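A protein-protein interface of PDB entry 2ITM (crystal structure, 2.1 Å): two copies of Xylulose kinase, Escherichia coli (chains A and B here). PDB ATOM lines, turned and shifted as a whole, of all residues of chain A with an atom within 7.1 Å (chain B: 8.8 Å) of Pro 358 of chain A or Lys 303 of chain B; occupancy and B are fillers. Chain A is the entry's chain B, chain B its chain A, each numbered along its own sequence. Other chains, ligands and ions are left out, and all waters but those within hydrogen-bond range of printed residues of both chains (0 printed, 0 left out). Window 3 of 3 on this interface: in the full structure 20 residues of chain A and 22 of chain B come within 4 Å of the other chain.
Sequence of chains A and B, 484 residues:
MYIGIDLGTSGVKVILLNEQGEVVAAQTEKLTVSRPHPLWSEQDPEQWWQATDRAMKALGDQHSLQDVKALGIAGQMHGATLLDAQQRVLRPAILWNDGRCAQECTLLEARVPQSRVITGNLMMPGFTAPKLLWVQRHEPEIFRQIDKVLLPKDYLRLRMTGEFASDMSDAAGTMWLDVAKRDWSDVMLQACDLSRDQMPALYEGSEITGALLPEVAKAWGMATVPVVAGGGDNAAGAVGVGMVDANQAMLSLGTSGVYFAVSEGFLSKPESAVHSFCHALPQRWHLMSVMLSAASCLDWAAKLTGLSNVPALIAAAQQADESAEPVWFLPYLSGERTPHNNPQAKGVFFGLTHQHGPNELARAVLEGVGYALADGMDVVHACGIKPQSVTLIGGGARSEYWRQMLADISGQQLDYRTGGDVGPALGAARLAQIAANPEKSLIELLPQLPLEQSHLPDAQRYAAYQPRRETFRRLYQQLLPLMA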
ATOM      1  N   THR A 305     -21.911 -25.041   9.941  1.00  0.00           N
ATOM      2  CA  THR A 305     -20.647 -24.857  10.626  1.00  0.00           C
ATOM      3  C   THR A 305     -19.564 -24.260   9.738  1.00  0.00           C
ATOM      4  O   THR A 305     -18.516 -23.870  10.217  1.00  0.00           O
ATOM      5  CB  THR A 305     -20.145 -26.181  11.193  1.00  0.00           C
ATOM      6  OG1 THR A 305     -20.319 -27.213  10.224  1.00  0.00           O
ATOM      7  CG2 THR A 305     -21.019 -26.631  12.349  1.00  0.00           C
ATOM      8  N   GLY A 306     -19.822 -24.216   8.438  1.00  0.00           N
ATOM      9  CA  GLY A 306     -18.809 -23.847   7.470  1.00  0.00           C
ATOM     10  C   GLY A 306     -17.783 -24.924   7.175  1.00  0.00           C
ATOM     11  O   GLY A 306     -16.715 -24.637   6.666  1.00  0.00           O
ATOM     12  N   LEU A 307     -18.106 -26.169   7.489  1.00  0.00           N
ATOM     13  CA  LEU A 307     -17.189 -27.266   7.238  1.00  0.00           C
ATOM     14  C   LEU A 307     -17.525 -28.007   5.958  1.00  0.00           C
ATOM     15  O   LEU A 307     -17.010 -29.082   5.703  1.00  0.00           O
ATOM     16  CB  LEU A 307     -17.158 -28.227   8.423  1.00  0.00           C
ATOM     17  CG  LEU A 307     -16.471 -27.730   9.690  1.00  0.00           C
ATOM     18  CD1 LEU A 307     -17.138 -28.278  10.906  1.00  0.00           C
ATOM     19  CD2 LEU A 307     -15.012 -28.086   9.685  1.00  0.00           C
ATOM     20  N   LEU A 313     -16.937 -32.646   8.662  1.00  0.00           N
ATOM     21  CA  LEU A 313     -17.679 -32.450   9.902  1.00  0.00           C
ATOM     22  C   LEU A 313     -17.381 -33.523  10.937  1.00  0.00           C
ATOM     23  O   LEU A 313     -17.141 -33.224  12.089  1.00  0.00           O
ATOM     24  CB  LEU A 313     -19.180 -32.369   9.645  1.00  0.00           C
ATOM     25  CG  LEU A 313     -20.015 -32.052  10.884  1.00  0.00           C
ATOM     26  CD1 LEU A 313     -20.384 -30.608  10.909  1.00  0.00           C
ATOM     27  CD2 LEU A 313     -21.243 -32.900  10.948  1.00  0.00           C
ATOM     28  N   ALA A 316     -13.775 -33.269  12.146  1.00  0.00           N
ATOM     29  CA  ALA A 316     -13.680 -32.210  13.121  1.00  0.00           C
ATOM     30  C   ALA A 316     -14.219 -32.631  14.483  1.00  0.00           C
ATOM     31  O   ALA A 316     -13.607 -32.359  15.503  1.00  0.00           O
ATOM     32  CB  ALA A 316     -14.372 -30.968  12.616  1.00  0.00           C
ATOM     33  N   ALA A 317     -15.361 -33.303  14.487  1.00  0.00           N
ATOM     34  CA  ALA A 317     -15.977 -33.748  15.725  1.00  0.00           C
ATOM     35  C   ALA A 317     -14.977 -34.530  16.553  1.00  0.00           C
ATOM     36  O   ALA A 317     -14.939 -34.418  17.766  1.00  0.00           O
ATOM     37  CB  ALA A 317     -17.181 -34.583  15.436  1.00  0.00           C
ATOM     38  N   ALA A 320     -12.594 -32.350  18.622  1.00  0.00           N
ATOM     39  CA  ALA A 320     -13.141 -31.582  19.732  1.00  0.00           C
ATOM     40  C   ALA A 320     -12.469 -31.974  21.033  1.00  0.00           C
ATOM     41  O   ALA A 320     -11.936 -33.060  21.153  1.00  0.00           O
ATOM     42  CB  ALA A 320     -14.640 -31.775  19.823  1.00  0.00           C
ATOM     43  N   HIS A 354     -17.442 -20.087  25.823  1.00  0.00           N
ATOM     44  CA  HIS A 354     -16.234 -19.623  25.193  1.00  0.00           C
ATOM     45  C   HIS A 354     -15.338 -20.764  24.728  1.00  0.00           C
ATOM     46  O   HIS A 354     -14.483 -20.572  23.885  1.00  0.00           O
ATOM     47  CB  HIS A 354     -15.502 -18.656  26.112  1.00  0.00           C
ATOM     48  CG  HIS A 354     -16.251 -17.385  26.353  1.00  0.00           C
ATOM     49  ND1 HIS A 354     -17.315 -16.992  25.574  1.00  0.00           N
ATOM     50  CD2 HIS A 354     -16.091 -16.418  27.290  1.00  0.00           C
ATOM     51  CE1 HIS A 354     -17.778 -15.838  26.010  1.00  0.00           C
ATOM     52  NE2 HIS A 354     -17.053 -15.468  27.049  1.00  0.00           N
ATOM     53  N   GLN A 355     -15.572 -21.960  25.255  1.00  0.00           N
ATOM     54  CA  GLN A 355     -14.742 -23.113  24.936  1.00  0.00           C
ATOM     55  C   GLN A 355     -15.156 -23.938  23.714  1.00  0.00           C
ATOM     56  O   GLN A 355     -14.708 -25.056  23.554  1.00  0.00           O
ATOM     57  CB  GLN A 355     -14.544 -24.010  26.162  1.00  0.00           C
ATOM     58  CG  GLN A 355     -15.812 -24.498  26.812  1.00  0.00           C
ATOM     59  CD  GLN A 355     -15.616 -24.930  28.249  1.00  0.00           C
ATOM     60  OE1 GLN A 355     -14.632 -24.575  28.878  1.00  0.00           O
ATOM     61  NE2 GLN A 355     -16.559 -25.690  28.769  1.00  0.00           N
ATOM     62  N   HIS A 356     -16.006 -23.380  22.864  1.00  0.00           N
ATOM     63  CA  HIS A 356     -16.714 -24.165  21.876  1.00  0.00           C
ATOM     64  C   HIS A 356     -16.381 -23.663  20.486  1.00  0.00           C
ATOM     65  O   HIS A 356     -16.831 -22.608  20.074  1.00  0.00           O
ATOM     66  CB  HIS A 356     -18.226 -24.101  22.098  1.00  0.00           C
ATOM     67  CG  HIS A 356     -18.688 -24.772  23.352  1.00  0.00           C
ATOM     68  ND1 HIS A 356     -18.191 -25.980  23.779  1.00  0.00           N
ATOM     69  CD2 HIS A 356     -19.611 -24.404  24.267  1.00  0.00           C
ATOM     70  CE1 HIS A 356     -18.782 -26.325  24.905  1.00  0.00           C
ATOM     71  NE2 HIS A 356     -19.647 -25.385  25.223  1.00  0.00           N
ATOM     72  N   GLY A 357     -15.580 -24.430  19.767  1.00  0.00           N
ATOM     73  CA  GLY A 357     -15.230 -24.081  18.413  1.00  0.00           C
ATOM     74  C   GLY A 357     -15.963 -24.969  17.453  1.00  0.00           C
ATOM     75  O   GLY A 357     -16.742 -25.809  17.853  1.00  0.00           O
ATOM     76  N   PRO A 358     -15.706 -24.784  16.171  1.00  0.00           N
ATOM     77  CA  PRO A 358     -16.316 -25.636  15.157  1.00  0.00           C
ATOM     78  C   PRO A 358     -16.139 -27.116  15.441  1.00  0.00           C
ATOM     79  O   PRO A 358     -16.986 -27.887  15.037  1.00  0.00           O
ATOM     80  CB  PRO A 358     -15.583 -25.228  13.891  1.00  0.00           C
ATOM     81  CG  PRO A 358     -15.274 -23.799  14.128  1.00  0.00           C
ATOM     82  CD  PRO A 358     -14.915 -23.702  15.567  1.00  0.00           C
ATOM     83  N   ASN A 359     -15.066 -27.499  16.122  1.00  0.00           N
ATOM     84  CA  ASN A 359     -14.917 -28.872  16.563  1.00  0.00           C
ATOM     85  C   ASN A 359     -16.031 -29.275  17.529  1.00  0.00           C
ATOM     86  O   ASN A 359     -16.819 -30.164  17.250  1.00  0.00           O
ATOM     87  CB  ASN A 359     -13.560 -29.102  17.226  1.00  0.00           C
ATOM     88  CG  ASN A 359     -12.383 -28.902  16.278  1.00  0.00           C
ATOM     89  OD1 ASN A 359     -12.538 -28.836  15.065  1.00  0.00           O
ATOM     90  ND2 ASN A 359     -11.197 -28.800  16.850  1.00  0.00           N
ATOM     91  N   GLU A 360     -16.059 -28.615  18.679  1.00  0.00           N
ATOM     92  CA  GLU A 360     -17.085 -28.837  19.680  1.00  0.00           C
ATOM     93  C   GLU A 360     -18.459 -28.833  19.049  1.00  0.00           C
ATOM     94  O   GLU A 360     -19.304 -29.650  19.367  1.00  0.00           O
ATOM     95  CB  GLU A 360     -17.004 -27.764  20.744  1.00  0.00           C
ATOM     96  CG  GLU A 360     -15.720 -27.779  21.538  1.00  0.00           C
ATOM     97  CD  GLU A 360     -14.477 -27.582  20.687  1.00  0.00           C
ATOM     98  OE1 GLU A 360     -13.439 -28.164  21.041  1.00  0.00           O
ATOM     99  OE2 GLU A 360     -14.538 -26.852  19.683  1.00  0.00           O
ATOM    100  N   LEU A 361     -18.659 -27.909  18.130  1.00  0.00           N
ATOM    101  CA  LEU A 361     -19.942 -27.724  17.513  1.00  0.00           C
ATOM    102  C   LEU A 361     -20.312 -28.954  16.701  1.00  0.00           C
ATOM    103  O   LEU A 361     -21.460 -29.361  16.658  1.00  0.00           O
ATOM    104  CB  LEU A 361     -19.906 -26.479  16.637  1.00  0.00           C
ATOM    105  CG  LEU A 361     -20.986 -25.416  16.794  1.00  0.00           C
ATOM    106  CD1 LEU A 361     -21.020 -24.843  18.172  1.00  0.00           C
ATOM    107  CD2 LEU A 361     -20.767 -24.343  15.774  1.00  0.00           C
ATOM    108  N   ALA A 362     -19.309 -29.547  16.067  1.00  0.00           N
ATOM    109  CA  ALA A 362     -19.494 -30.725  15.244  1.00  0.00           C
ATOM    110  C   ALA A 362     -19.827 -31.943  16.082  1.00  0.00           C
ATOM    111  O   ALA A 362     -20.704 -32.704  15.742  1.00  0.00           O
ATOM    112  CB  ALA A 362     -18.268 -30.981  14.410  1.00  0.00           C
ATOM    113  N   ARG A 363     -19.117 -32.108  17.182  1.00  0.00           N
ATOM    114  CA  ARG A 363     -19.428 -33.143  18.149  1.00  0.00           C
ATOM    115  C   ARG A 363     -20.871 -33.030  18.620  1.00  0.00           C
ATOM    116  O   ARG A 363     -21.542 -34.014  18.759  1.00  0.00           O
ATOM    117  CB  ARG A 363     -18.480 -33.053  19.333  1.00  0.00           C
ATOM    118  CG  ARG A 363     -18.543 -34.202  20.260  1.00  0.00           C
ATOM    119  CD  ARG A 363     -17.420 -35.174  20.085  1.00  0.00           C
ATOM    120  NE  ARG A 363     -16.670 -35.373  21.310  1.00  0.00           N
ATOM    121  CZ  ARG A 363     -15.395 -35.725  21.353  1.00  0.00           C
ATOM    122  NH1 ARG A 363     -14.709 -35.908  20.239  1.00  0.00           N
ATOM    123  NH2 ARG A 363     -14.799 -35.885  22.519  1.00  0.00           N
ATOM    124  N   ALA A 364     -21.331 -31.810  18.841  1.00  0.00           N
ATOM    125  CA  ALA A 364     -22.683 -31.575  19.326  1.00  0.00           C
ATOM    126  C   ALA A 364     -23.739 -31.944  18.300  1.00  0.00           C
ATOM    127  O   ALA A 364     -24.791 -32.404  18.630  1.00  0.00           O
ATOM    128  CB  ALA A 364     -22.852 -30.150  19.777  1.00  0.00           C
ATOM    129  N   SER B 296     -14.461 -10.756  24.854  1.00  0.00           N
ATOM    130  CA  SER B 296     -14.341 -12.194  24.941  1.00  0.00           C
ATOM    131  C   SER B 296     -15.485 -12.895  24.221  1.00  0.00           C
ATOM    132  O   SER B 296     -15.497 -14.122  24.133  1.00  0.00           O
ATOM    133  CB  SER B 296     -14.241 -12.627  26.409  1.00  0.00           C
ATOM    134  OG  SER B 296     -14.777 -13.929  26.564  1.00  0.00           O
ATOM    135  N   CYS B 297     -16.420 -12.126  23.685  1.00  0.00           N
ATOM    136  CA  CYS B 297     -17.486 -12.691  22.865  1.00  0.00           C
ATOM    137  C   CYS B 297     -17.122 -12.646  21.384  1.00  0.00           C
ATOM    138  O   CYS B 297     -17.093 -13.669  20.716  1.00  0.00           O
ATOM    139  CB  CYS B 297     -18.806 -11.970  23.125  1.00  0.00           C
ATOM    140  SG  CYS B 297     -19.695 -12.523  24.597  1.00  0.00           S
ATOM    141  N   LEU B 298     -16.806 -11.449  20.902  1.00  0.00           N
ATOM    142  CA  LEU B 298     -16.328 -11.232  19.545  1.00  0.00           C
ATOM    143  C   LEU B 298     -15.200 -12.174  19.147  1.00  0.00           C
ATOM    144  O   LEU B 298     -15.203 -12.731  18.063  1.00  0.00           O
ATOM    145  CB  LEU B 298     -15.860  -9.797  19.370  1.00  0.00           C
ATOM    146  CG  LEU B 298     -16.913  -8.704  19.328  1.00  0.00           C
ATOM    147  CD1 LEU B 298     -16.359  -7.474  18.638  1.00  0.00           C
ATOM    148  CD2 LEU B 298     -18.186  -9.183  18.660  1.00  0.00           C
ATOM    149  N   ASP B 299     -14.233 -12.332  20.028  1.00  0.00           N
ATOM    150  CA  ASP B 299     -13.170 -13.284  19.789  1.00  0.00           C
ATOM    151  C   ASP B 299     -13.725 -14.678  19.578  1.00  0.00           C
ATOM    152  O   ASP B 299     -13.165 -15.475  18.839  1.00  0.00           O
ATOM    153  CB  ASP B 299     -12.170 -13.270  20.936  1.00  0.00           C
ATOM    154  CG  ASP B 299     -11.286 -12.055  20.914  1.00  0.00           C
ATOM    155  OD1 ASP B 299     -10.860 -11.623  21.991  1.00  0.00           O
ATOM    156  OD2 ASP B 299     -10.966 -11.457  19.873  1.00  0.00           O
ATOM    157  N   TRP B 300     -14.836 -14.966  20.238  1.00  0.00           N
ATOM    158  CA  TRP B 300     -15.363 -16.318  20.263  1.00  0.00           C
ATOM    159  C   TRP B 300     -16.188 -16.580  19.013  1.00  0.00           C
ATOM    160  O   TRP B 300     -15.939 -17.547  18.308  1.00  0.00           O
ATOM    161  CB  TRP B 300     -16.155 -16.570  21.548  1.00  0.00           C
ATOM    162  CG  TRP B 300     -17.020 -17.777  21.523  1.00  0.00           C
ATOM    163  CD1 TRP B 300     -16.675 -19.039  21.874  1.00  0.00           C
ATOM    164  CD2 TRP B 300     -18.390 -17.830  21.145  1.00  0.00           C
ATOM    165  NE1 TRP B 300     -17.745 -19.882  21.732  1.00  0.00           N
ATOM    166  CE2 TRP B 300     -18.811 -19.159  21.278  1.00  0.00           C
ATOM    167  CE3 TRP B 300     -19.316 -16.879  20.699  1.00  0.00           C
ATOM    168  CZ2 TRP B 300     -20.103 -19.564  20.979  1.00  0.00           C
ATOM    169  CZ3 TRP B 300     -20.594 -17.284  20.399  1.00  0.00           C
ATOM    170  CH2 TRP B 300     -20.981 -18.605  20.544  1.00  0.00           C
ATOM    171  N   ALA B 301     -17.135 -15.696  18.724  1.00  0.00           N
ATOM    172  CA  ALA B 301     -17.759 -15.657  17.414  1.00  0.00           C
ATOM    173  C   ALA B 301     -16.840 -15.825  16.218  1.00  0.00           C
ATOM    174  O   ALA B 301     -17.238 -16.353  15.196  1.00  0.00           O
ATOM    175  CB  ALA B 301     -18.456 -14.332  17.191  1.00  0.00           C
ATOM    176  N   ALA B 302     -15.604 -15.379  16.379  1.00  0.00           N
ATOM    177  CA  ALA B 302     -14.585 -15.542  15.363  1.00  0.00           C
ATOM    178  C   ALA B 302     -14.132 -16.978  15.286  1.00  0.00           C
ATOM    179  O   ALA B 302     -14.241 -17.609  14.249  1.00  0.00           O
ATOM    180  CB  ALA B 302     -13.413 -14.630  15.637  1.00  0.00           C
ATOM    181  N   LYS B 303     -13.630 -17.504  16.388  1.00  0.00           N
ATOM    182  CA  LYS B 303     -13.051 -18.834  16.349  1.00  0.00           C
ATOM    183  C   LYS B 303     -14.097 -19.918  16.195  1.00  0.00           C
ATOM    184  O   LYS B 303     -13.901 -20.852  15.439  1.00  0.00           O
ATOM    185  CB  LYS B 303     -12.185 -19.107  17.572  1.00  0.00           C
ATOM    186  CG  LYS B 303     -12.295 -20.535  18.102  1.00  0.00           C
ATOM    187  CD  LYS B 303     -11.740 -21.551  17.108  1.00  0.00           C
ATOM    188  CE  LYS B 303     -10.844 -22.570  17.788  1.00  0.00           C
ATOM    189  NZ  LYS B 303     -10.945 -22.485  19.260  1.00  0.00           N
ATOM    190  N   LEU B 304     -15.191 -19.794  16.924  1.00  0.00           N
ATOM    191  CA  LEU B 304     -16.436 -20.456  16.572  1.00  0.00           C
ATOM    192  C   LEU B 304     -16.816 -20.669  15.116  1.00  0.00           C
ATOM    193  O   LEU B 304     -17.207 -21.763  14.729  1.00  0.00           O
ATOM    194  CB  LEU B 304     -17.621 -19.656  17.097  1.00  0.00           C
ATOM    195  CG  LEU B 304     -18.911 -20.416  17.382  1.00  0.00           C
ATOM    196  CD1 LEU B 304     -18.685 -21.605  18.267  1.00  0.00           C
ATOM    197  CD2 LEU B 304     -19.906 -19.493  18.006  1.00  0.00           C
ATOM    198  N   THR B 305     -16.720 -19.608  14.320  1.00  0.00           N
ATOM    199  CA  THR B 305     -17.159 -19.654  12.935  1.00  0.00           C
ATOM    200  C   THR B 305     -15.895 -19.942  12.149  1.00  0.00           C
ATOM    201  O   THR B 305     -15.880 -19.863  10.929  1.00  0.00           O
ATOM    202  CB  THR B 305     -17.843 -18.376  12.420  1.00  0.00           C
ATOM    203  OG1 THR B 305     -17.049 -17.231  12.726  1.00  0.00           O
ATOM    204  CG2 THR B 305     -19.119 -18.123  13.169  1.00  0.00           C
ATOM    205  N   GLY B 306     -14.837 -20.283  12.865  1.00  0.00           N
ATOM    206  CA  GLY B 306     -13.571 -20.602  12.251  1.00  0.00           C
ATOM    207  C   GLY B 306     -12.982 -19.445  11.489  1.00  0.00           C
ATOM    208  O   GLY B 306     -11.951 -19.582  10.848  1.00  0.00           O
ATOM    209  N   LEU B 307     -13.639 -18.299  11.569  1.00  0.00           N
ATOM    210  CA  LEU B 307     -13.035 -17.042  11.166  1.00  0.00           C
ATOM    211  C   LEU B 307     -11.802 -16.708  11.986  1.00  0.00           C
ATOM    212  O   LEU B 307     -11.678 -17.124  13.131  1.00  0.00           O
ATOM    213  CB  LEU B 307     -14.055 -15.921  11.270  1.00  0.00           C
ATOM    214  CG  LEU B 307     -15.230 -16.199  10.351  1.00  0.00           C
ATOM    215  CD1 LEU B 307     -16.136 -15.015  10.192  1.00  0.00           C
ATOM    216  CD2 LEU B 307     -14.681 -16.646   9.028  1.00  0.00           C
ATOM    217  N   SER B 308     -10.892 -15.954  11.392  1.00  0.00           N
ATOM    218  CA  SER B 308      -9.503 -15.935  11.825  1.00  0.00           C
ATOM    219  C   SER B 308      -9.293 -14.879  12.899  1.00  0.00           C
ATOM    220  O   SER B 308      -8.609 -15.103  13.891  1.00  0.00           O
ATOM    221  CB  SER B 308      -8.595 -15.641  10.635  1.00  0.00           C
ATOM    222  OG  SER B 308      -7.241 -15.902  10.947  1.00  0.00           O
ATOM    223  N   ASN B 309      -9.903 -13.726  12.689  1.00  0.00           N
ATOM    224  CA  ASN B 309      -9.585 -12.540  13.450  1.00  0.00           C
ATOM    225  C   ASN B 309     -10.815 -11.659  13.535  1.00  0.00           C
ATOM    226  O   ASN B 309     -11.798 -11.880  12.837  1.00  0.00           O
ATOM    227  CB  ASN B 309      -8.451 -11.779  12.775  1.00  0.00           C
ATOM    228  CG  ASN B 309      -8.734 -11.510  11.322  1.00  0.00           C
ATOM    229  OD1 ASN B 309      -8.585 -12.376  10.474  1.00  0.00           O
ATOM    230  ND2 ASN B 309      -9.160 -10.297  11.027  1.00  0.00           N
ATOM    231  N   VAL B 310     -10.765 -10.666  14.404  1.00  0.00           N
ATOM    232  CA  VAL B 310     -11.980 -10.009  14.812  1.00  0.00           C
ATOM    233  C   VAL B 310     -12.540  -9.191  13.672  1.00  0.00           C
ATOM    234  O   VAL B 310     -13.630  -8.643  13.764  1.00  0.00           O
ATOM    235  CB  VAL B 310     -11.791  -9.158  16.050  1.00  0.00           C
ATOM    236  CG1 VAL B 310     -12.649  -7.949  15.964  1.00  0.00           C
ATOM    237  CG2 VAL B 310     -12.157  -9.942  17.268  1.00  0.00           C
ATOM    238  N   ALA B 312     -11.918 -10.364  10.100  1.00  0.00           N
ATOM    239  CA  ALA B 312     -12.536 -11.422   9.318  1.00  0.00           C
ATOM    240  C   ALA B 312     -13.998 -11.460   9.693  1.00  0.00           C
ATOM    241  O   ALA B 312     -14.879 -11.306   8.865  1.00  0.00           O
ATOM    242  CB  ALA B 312     -11.881 -12.729   9.588  1.00  0.00           C
ATOM    243  N   LEU B 313     -14.244 -11.660  10.969  1.00  0.00           N
ATOM    244  CA  LEU B 313     -15.594 -11.810  11.448  1.00  0.00           C
ATOM    245  C   LEU B 313     -16.441 -10.637  10.991  1.00  0.00           C
ATOM    246  O   LEU B 313     -17.381 -10.804  10.240  1.00  0.00           O
ATOM    247  CB  LEU B 313     -15.592 -11.907  12.962  1.00  0.00           C
ATOM    248  CG  LEU B 313     -16.942 -11.660  13.596  1.00  0.00           C
ATOM    249  CD1 LEU B 313     -17.769 -12.899  13.491  1.00  0.00           C
ATOM    250  CD2 LEU B 313     -16.766 -11.263  15.022  1.00  0.00           C
ATOM    251  N   PRO B 358     -22.008 -19.345   8.082  1.00  0.00           N
ATOM    252  CA  PRO B 358     -21.170 -18.632   9.042  1.00  0.00           C
ATOM    253  C   PRO B 358     -21.340 -17.122   9.000  1.00  0.00           C
ATOM    254  O   PRO B 358     -21.191 -16.474  10.012  1.00  0.00           O
ATOM    255  CB  PRO B 358     -19.767 -19.007   8.606  1.00  0.00           C
ATOM    256  CG  PRO B 358     -19.923 -20.292   7.951  1.00  0.00           C
ATOM    257  CD  PRO B 358     -21.215 -20.246   7.236  1.00  0.00           C
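Of the 18 printed residues of chain A, 5 touch a printed residue of chain B.
Printed residues of chain A that touch a printed residue of chain B: Gly 306, His 354, His 356, Pro 358 and Leu 361.
Hydrophobic or aromatic side chains of chain A within 4 Å of the printed part of chain B: His 354, Pro 358 and Leu 361.
Of the 18 printed residues of chain B, 6 touch a printed residue of chain A.
Hydrophobic or aromatic side chains of chain B within 4 Å of the printed part of chain A: Trp 300, Leu 304 and Pro 358.
Among the printed residues, 9 pairs touch across the chains.
Among the printed residues, no Asp or Glu carboxylate lies within 4 Å of a Lys or Arg side-chain nitrogen of the other chain.
The backbone carbonyl oxygen (O) of His 356 of chain A lies within hydrogen-bond range of the indole nitrogen (NE1) of Trp 300 of chain B, at 3.3 Å.
The side-chain hydroxyl (OG) of Ser 296 of chain B is in hydrogen-bond range of a ring nitrogen (NE2) of His 354 of chain A (2.8 Å).
Of the printed residues of chain B, Pro 358 of chain A touches Lys 303 (3.0 Å), Leu 304 (2.9 Å) and Gly 306 (3.8 Å).
Lys 303 of chain B touches one residue of chain A.
No residue of chain B comes within 4 Å of Gly 357 of chain A.
Of the printed residues of chain A, Gly 306 of chain B touches Pro 358.
Printed residues of chain B within 4 Å of His 356 of chain A: Trp 300 and Leu 304.
Of the printed residues of chain B, Leu 361 of chain A touches Leu 304.
Of the printed residues of chain A, Trp 300 of chain B touches His 354 (3.3 Å) and His 356 (3.3 Å).
Printed residues of chain A within 4 Å of Pro 358 of chain B: Gly 306.
The nearest residue of chain B that does not touch Pro 358 of chain A is Thr 305 of chain B (4.4 Å).
The nearest residue of chain A that does not touch Lys 303 of chain B is Gly 357 of chain A (4.5 Å).
The nearest printed residue of chain A that does not touch Ser 296 of chain B is Gln 355 of chain A (7.9 Å).
Gly 306 of chain A touches Pro 358 of chain B, and with the chains exchanged Pro 358 of chain A touches Gly 306 of chain B.
Positions printed for both chains: 305, 306, 307, 313 and 358.
Of the 9 pairs that touch across the chains among the printed residues, 2 have their exchanged pair printed and touching as well.
Among the printed residues, pairs that only touch across the chains: His 356 of chain A with Leu 304 of chain B (2.8 Å), Pro 358 of chain A with Leu 304 of chain B (2.9 Å), Pro 358 of chain A with Lys 303 of chain B (3.0 Å), His 354 of chain A with Trp 300 of chain B (3.3 Å), Gly 306 of chain A with Pro 358 of chain B (3.8 Å), Pro 358 of chain A with Gly 306 of chain B (3.8 Å) and Leu 361 of chain A with Leu 304 of chain B (3.99 Å).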
